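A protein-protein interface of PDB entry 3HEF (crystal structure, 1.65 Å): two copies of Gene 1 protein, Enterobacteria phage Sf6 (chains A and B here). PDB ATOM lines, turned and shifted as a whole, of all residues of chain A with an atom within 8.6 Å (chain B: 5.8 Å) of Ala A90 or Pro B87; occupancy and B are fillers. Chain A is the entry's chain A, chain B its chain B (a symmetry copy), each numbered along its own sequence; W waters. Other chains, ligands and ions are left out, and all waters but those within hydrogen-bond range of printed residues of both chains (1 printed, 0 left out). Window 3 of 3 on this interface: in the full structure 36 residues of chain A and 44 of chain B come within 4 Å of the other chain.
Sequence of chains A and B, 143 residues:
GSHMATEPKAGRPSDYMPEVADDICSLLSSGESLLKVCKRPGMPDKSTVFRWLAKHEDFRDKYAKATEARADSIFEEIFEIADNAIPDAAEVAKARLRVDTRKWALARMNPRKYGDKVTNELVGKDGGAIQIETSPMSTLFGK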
ATOM      1  N   ALA A  85      10.848  -0.024  -8.396  1.00  0.00           N
ATOM      2  CA  ALA A  85      11.671  -0.365  -9.548  1.00  0.00           C
ATOM      3  C   ALA A  85      11.981   0.896 -10.369  1.00  0.00           C
ATOM      4  O   ALA A  85      11.110   1.730 -10.579  1.00  0.00           O
ATOM      5  CB  ALA A  85      10.946  -1.377 -10.440  1.00  0.00           C
ATOM      6  N   ILE A  86      13.216   1.009 -10.836  1.00  0.00           N
ATOM      7  CA  ILE A  86      13.592   2.148 -11.675  1.00  0.00           C
ATOM      8  C   ILE A  86      12.907   1.925 -13.029  1.00  0.00           C
ATOM      9  O   ILE A  86      13.048   0.850 -13.645  1.00  0.00           O
ATOM     10  CB  ILE A  86      15.128   2.201 -11.844  1.00  0.00           C
ATOM     11  CG1 ILE A  86      15.780   2.492 -10.483  1.00  0.00           C
ATOM     12  CG2 ILE A  86      15.498   3.216 -12.923  1.00  0.00           C
ATOM     13  CD1 ILE A  86      17.281   2.270 -10.432  1.00  0.00           C
ATOM     14  N   PRO A  87      12.144   2.924 -13.513  1.00  0.00           N
ATOM     15  CA  PRO A  87      11.438   2.811 -14.787  1.00  0.00           C
ATOM     16  C   PRO A  87      12.309   2.837 -16.046  1.00  0.00           C
ATOM     17  O   PRO A  87      12.195   3.719 -16.909  1.00  0.00           O
ATOM     18  CB  PRO A  87      10.415   3.949 -14.709  1.00  0.00           C
ATOM     19  CG  PRO A  87      11.148   4.985 -13.940  1.00  0.00           C
ATOM     20  CD  PRO A  87      11.811   4.192 -12.839  1.00  0.00           C
ATOM     21  N   ASP A  88      13.183   1.843 -16.120  1.00  0.00           N
ATOM     22  CA  ASP A  88      14.091   1.613 -17.229  1.00  0.00           C
ATOM     23  C   ASP A  88      13.851   0.150 -17.621  1.00  0.00           C
ATOM     24  O   ASP A  88      13.658  -0.690 -16.745  1.00  0.00           O
ATOM     25  CB  ASP A  88      15.525   1.798 -16.761  1.00  0.00           C
ATOM     26  CG  ASP A  88      16.508   1.052 -17.622  1.00  0.00           C
ATOM     27  OD1 ASP A  88      16.752   1.501 -18.766  1.00  0.00           O
ATOM     28  OD2 ASP A  88      17.029   0.010 -17.162  1.00  0.00           O
ATOM     29  N   ALA A  89      13.875  -0.159 -18.913  1.00  0.00           N
ATOM     30  CA  ALA A  89      13.607  -1.528 -19.373  1.00  0.00           C
ATOM     31  C   ALA A  89      14.353  -2.649 -18.650  1.00  0.00           C
ATOM     32  O   ALA A  89      13.727  -3.591 -18.132  1.00  0.00           O
ATOM     33  CB  ALA A  89      13.857  -1.633 -20.881  1.00  0.00           C
ATOM     34  N   ALA A  90      15.676  -2.579 -18.620  1.00  0.00           N
ATOM     35  CA  ALA A  90      16.451  -3.632 -17.971  1.00  0.00           C
ATOM     36  C   ALA A  90      16.236  -3.670 -16.471  1.00  0.00           C
ATOM     37  O   ALA A  90      16.203  -4.754 -15.870  1.00  0.00           O
ATOM     38  CB  ALA A  90      17.929  -3.467 -18.280  1.00  0.00           C
ATOM     39  N   GLU A  91      16.107  -2.500 -15.851  1.00  0.00           N
ATOM     40  CA  GLU A  91      15.892  -2.464 -14.414  1.00  0.00           C
ATOM     41  C   GLU A  91      14.518  -3.049 -14.073  1.00  0.00           C
ATOM     42  O   GLU A  91      14.390  -3.746 -13.083  1.00  0.00           O
ATOM     43  CB  GLU A  91      15.975  -1.047 -13.854  1.00  0.00           C
ATOM     44  CG  GLU A  91      17.376  -0.430 -13.872  1.00  0.00           C
ATOM     45  CD  GLU A  91      18.376  -1.082 -12.923  1.00  0.00           C
ATOM     46  OE1 GLU A  91      18.024  -2.015 -12.156  1.00  0.00           O
ATOM     47  OE2 GLU A  91      19.551  -0.651 -12.940  1.00  0.00           O
ATOM     48  N   VAL A  92      13.496  -2.756 -14.869  1.00  0.00           N
ATOM     49  CA  VAL A  92      12.173  -3.320 -14.567  1.00  0.00           C
ATOM     50  C   VAL A  92      12.246  -4.826 -14.790  1.00  0.00           C
ATOM     51  O   VAL A  92      11.655  -5.580 -14.014  1.00  0.00           O
ATOM     52  CB  VAL A  92      11.044  -2.743 -15.451  1.00  0.00           C
ATOM     53  CG1 VAL A  92       9.670  -3.393 -15.056  1.00  0.00           C
ATOM     54  CG2 VAL A  92      10.950  -1.244 -15.251  1.00  0.00           C
ATOM     55  N   ALA A  93      12.943  -5.262 -15.844  1.00  0.00           N
ATOM     56  CA  ALA A  93      13.103  -6.701 -16.115  1.00  0.00           C
ATOM     57  C   ALA A  93      13.814  -7.368 -14.933  1.00  0.00           C
ATOM     58  O   ALA A  93      13.456  -8.480 -14.528  1.00  0.00           O
ATOM     59  CB  ALA A  93      13.899  -6.928 -17.417  1.00  0.00           C
ATOM     60  N   LYS A  94      14.835  -6.711 -14.379  1.00  0.00           N
ATOM     61  CA  LYS A  94      15.548  -7.282 -13.238  1.00  0.00           C
ATOM     62  C   LYS A  94      14.648  -7.360 -12.009  1.00  0.00           C
ATOM     63  O   LYS A  94      14.640  -8.368 -11.296  1.00  0.00           O
ATOM     64  CB  LYS A  94      16.784  -6.458 -12.896  1.00  0.00           C
ATOM     65  CG  LYS A  94      17.466  -6.911 -11.643  1.00  0.00           C
ATOM     66  CD  LYS A  94      18.815  -6.172 -11.447  1.00  0.00           C
ATOM     67  CE  LYS A  94      19.430  -6.564 -10.129  1.00  0.00           C
ATOM     68  NZ  LYS A  94      20.813  -5.936  -9.923  1.00  0.00           N
ATOM     69  N   ALA A  95      13.880  -6.300 -11.784  1.00  0.00           N
ATOM     70  CA  ALA A  95      12.943  -6.237 -10.654  1.00  0.00           C
ATOM     71  C   ALA A  95      11.937  -7.384 -10.791  1.00  0.00           C
ATOM     72  O   ALA A  95      11.626  -8.055  -9.790  1.00  0.00           O
ATOM     73  CB  ALA A  95      12.207  -4.910 -10.654  1.00  0.00           C
ATOM     74  N   ARG A  96      11.432  -7.591 -12.005  1.00  0.00           N
ATOM     75  CA  ARG A  96      10.458  -8.693 -12.247  1.00  0.00           C
ATOM     76  C   ARG A  96      11.107 -10.040 -11.914  1.00  0.00           C
ATOM     77  O   ARG A  96      10.487 -10.929 -11.272  1.00  0.00           O
ATOM     78  CB  ARG A  96       9.999  -8.700 -13.708  1.00  0.00           C
ATOM     79  CG  ARG A  96       8.883  -9.710 -14.009  1.00  0.00           C
ATOM     80  CD  ARG A  96       8.478  -9.614 -15.479  1.00  0.00           C
ATOM     81  NE  ARG A  96       7.486 -10.622 -15.859  1.00  0.00           N
ATOM     82  CZ  ARG A  96       7.181 -10.929 -17.121  1.00  0.00           C
ATOM     83  NH1 ARG A  96       7.792 -10.313 -18.132  1.00  0.00           N
ATOM     84  NH2 ARG A  96       6.259 -11.849 -17.378  1.00  0.00           N
ATOM     85  N   LEU A  97      12.362 -10.214 -12.317  1.00  0.00           N
ATOM     86  CA  LEU A  97      13.055 -11.468 -12.025  1.00  0.00           C
ATOM     87  C   LEU A  97      13.251 -11.612 -10.504  1.00  0.00           C
ATOM     88  O   LEU A  97      13.064 -12.693  -9.939  1.00  0.00           O
ATOM     89  CB  LEU A  97      14.405 -11.512 -12.769  1.00  0.00           C
ATOM     90  CG  LEU A  97      15.266 -12.743 -12.413  1.00  0.00           C
ATOM     91  CD1 LEU A  97      14.528 -14.015 -12.803  1.00  0.00           C
ATOM     92  CD2 LEU A  97      16.613 -12.676 -13.191  1.00  0.00           C
ATOM     93  N   ALA B  85      22.050  -9.627 -10.885  1.00  0.00           N
ATOM     94  CA  ALA B  85      22.020  -9.570 -12.335  1.00  0.00           C
ATOM     95  C   ALA B  85      22.489  -8.199 -12.842  1.00  0.00           C
ATOM     96  O   ALA B  85      22.063  -7.173 -12.325  1.00  0.00           O
ATOM     97  CB  ALA B  85      20.585  -9.837 -12.838  1.00  0.00           C
ATOM     98  N   ILE B  86      23.358  -8.191 -13.844  1.00  0.00           N
ATOM     99  CA  ILE B  86      23.808  -6.913 -14.416  1.00  0.00           C
ATOM    100  C   ILE B  86      22.562  -6.313 -15.068  1.00  0.00           C
ATOM    101  O   ILE B  86      21.913  -6.981 -15.877  1.00  0.00           O
ATOM    102  CB  ILE B  86      24.867  -7.138 -15.509  1.00  0.00           C
ATOM    103  CG1 ILE B  86      26.124  -7.759 -14.902  1.00  0.00           C
ATOM    104  CG2 ILE B  86      25.182  -5.814 -16.208  1.00  0.00           C
ATOM    105  CD1 ILE B  86      27.057  -8.389 -15.943  1.00  0.00           C
ATOM    106  N   PRO B  87      22.216  -5.047 -14.749  1.00  0.00           N
ATOM    107  CA  PRO B  87      21.021  -4.444 -15.344  1.00  0.00           C
ATOM    108  C   PRO B  87      21.151  -4.074 -16.807  1.00  0.00           C
ATOM    109  O   PRO B  87      21.072  -2.903 -17.171  1.00  0.00           O
ATOM    110  CB  PRO B  87      20.757  -3.234 -14.448  1.00  0.00           C
ATOM    111  CG  PRO B  87      22.147  -2.828 -14.038  1.00  0.00           C
ATOM    112  CD  PRO B  87      22.800  -4.152 -13.728  1.00  0.00           C
ATOM    113  N   ASP B  88      21.353  -5.100 -17.627  1.00  0.00           N
ATOM    114  CA  ASP B  88      21.469  -4.986 -19.075  1.00  0.00           C
ATOM    115  C   ASP B  88      20.476  -5.998 -19.639  1.00  0.00           C
ATOM    116  O   ASP B  88      20.401  -7.114 -19.136  1.00  0.00           O
ATOM    117  CB  ASP B  88      22.868  -5.361 -19.525  1.00  0.00           C
ATOM    118  CG  ASP B  88      22.913  -5.738 -20.980  1.00  0.00           C
ATOM    119  OD1 ASP B  88      22.660  -4.851 -21.826  1.00  0.00           O
ATOM    120  OD2 ASP B  88      23.183  -6.925 -21.280  1.00  0.00           O
ATOM    121  N   ALA B  89      19.748  -5.626 -20.690  1.00  0.00           N
ATOM    122  CA  ALA B  89      18.727  -6.511 -21.261  1.00  0.00           C
ATOM    123  C   ALA B  89      19.137  -7.970 -21.445  1.00  0.00           C
ATOM    124  O   ALA B  89      18.484  -8.873 -20.913  1.00  0.00           O
ATOM    125  CB  ALA B  89      18.221  -5.946 -22.573  1.00  0.00           C
ATOM    126  N   GLU B  91      21.801  -9.533 -20.285  1.00  0.00           N
ATOM    127  CA  GLU B  91      22.294 -10.084 -19.049  1.00  0.00           C
ATOM    128  C   GLU B  91      21.110 -10.461 -18.140  1.00  0.00           C
ATOM    129  O   GLU B  91      21.171 -11.471 -17.441  1.00  0.00           O
ATOM    130  CB  GLU B  91      23.192  -9.085 -18.324  1.00  0.00           C
ATOM    131  CG  GLU B  91      24.577  -8.871 -18.971  1.00  0.00           C
ATOM    132  CD  GLU B  91      25.531 -10.066 -18.844  1.00  0.00           C
ATOM    133  OE1 GLU B  91      25.223 -11.058 -18.154  1.00  0.00           O
ATOM    134  OE2 GLU B  91      26.626 -10.016 -19.445  1.00  0.00           O
ATOM    135  N   VAL B  92      20.057  -9.649 -18.143  1.00  0.00           N
ATOM    136  CA  VAL B  92      18.903  -9.973 -17.291  1.00  0.00           C
ATOM    137  C   VAL B  92      18.200 -11.196 -17.866  1.00  0.00           C
ATOM    138  O   VAL B  92      17.769 -12.081 -17.104  1.00  0.00           O
ATOM    139  CB  VAL B  92      17.924  -8.791 -17.179  1.00  0.00           C
ATOM    140  CG1 VAL B  92      16.634  -9.205 -16.407  1.00  0.00           C
ATOM    141  CG2 VAL B  92      18.597  -7.662 -16.405  1.00  0.00           C
HETATM  142  O   HOH W   1      19.632  -0.176 -17.493  1.00  0.00           O
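The side-chain amino group (NZ) of Lys A94 is in hydrogen-bond range of the backbone carbonyl oxygen (O) of Ala B85 (3.0 Å).
OD2 of Asp A88 sits at hydrogen-bond distance from N of Ala A90, at 3.3 Å.
OD2 of Asp A88 is in hydrogen-bond range of N of Glu A91 (3.0 Å).
The backbone NH (N) of Glu B91 is in hydrogen-bond range of the side-chain carboxylate (OD2) of Asp B88 (3.1 Å).
Among the printed residues, merely in contact across the chains: Glu A91 with Pro B87 (3.2 Å), Ala A90 with Pro B87 (3.4 Å), Ala A93 with Val B92 (3.7 Å), Lys A94 with Val B92 (3.7 Å), Ala A90 with Ala B89 (3.7 Å), Ala A90 with Val B92 (3.8 Å) and Ala A90 with Asp B88 (3.8 Å).
Ala A90 touches just these residues of chain B: Pro B87 (3.4 Å), Asp B88 (3.8 Å), Ala B89 (3.7 Å) and Val B92 (3.8 Å).
Printed residues of chain A within 4 Å of Pro B87: Ala A90 (3.4 Å) and Glu A91 (3.2 Å).
Of the printed residues of chain A, Val B92 touches Ala A90, Ala A93 and Lys A94.
Of the printed residues of chain A, Ala B85 touches Lys A94.
Printed residues of chain B within 4 Å of Ala A93: Val B92.
Of the printed residues of chain B, Glu A91 touches Pro B87.
Asp A88 touches none of the printed residues of chain B.
The nearest printed residue of chain B that does not touch Ala A90 is Ile B86 (5.8 Å).
The nearest residue of chain A that does not touch Pro B87 is Lys A94 (4.6 Å).
The nearest printed residue of chain A that does not touch Asp B88 is Glu A91 (6.1 Å).
Of the 7 printed residues of chain B, 5 touch a printed residue of chain A.
Hydrophobic or aromatic side chains of chain B that line the printed part of chain A: Pro B87 and Val B92.
Of the 13 printed residues of chain A, 4 touch a printed residue of chain B.
Hydrophobic or aromatic side chains of chain A within 4 Å of the printed part of chain B: Ala A90 and Ala A93.
Glu A91 touches Pro B87, but with the chains exchanged Pro A87 does not touch Glu B91 (16.1 Å).
7 positions are printed for both chains.
Of the 8 pairs that touch across the chains among the printed residues, none has its exchanged pair printed and touching as well.
Water W1 bridges the side-chain carboxylate of Asp A88 (2.6 Å) and the backbone carbonyl oxygen of Pro B87 (3.1 Å).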
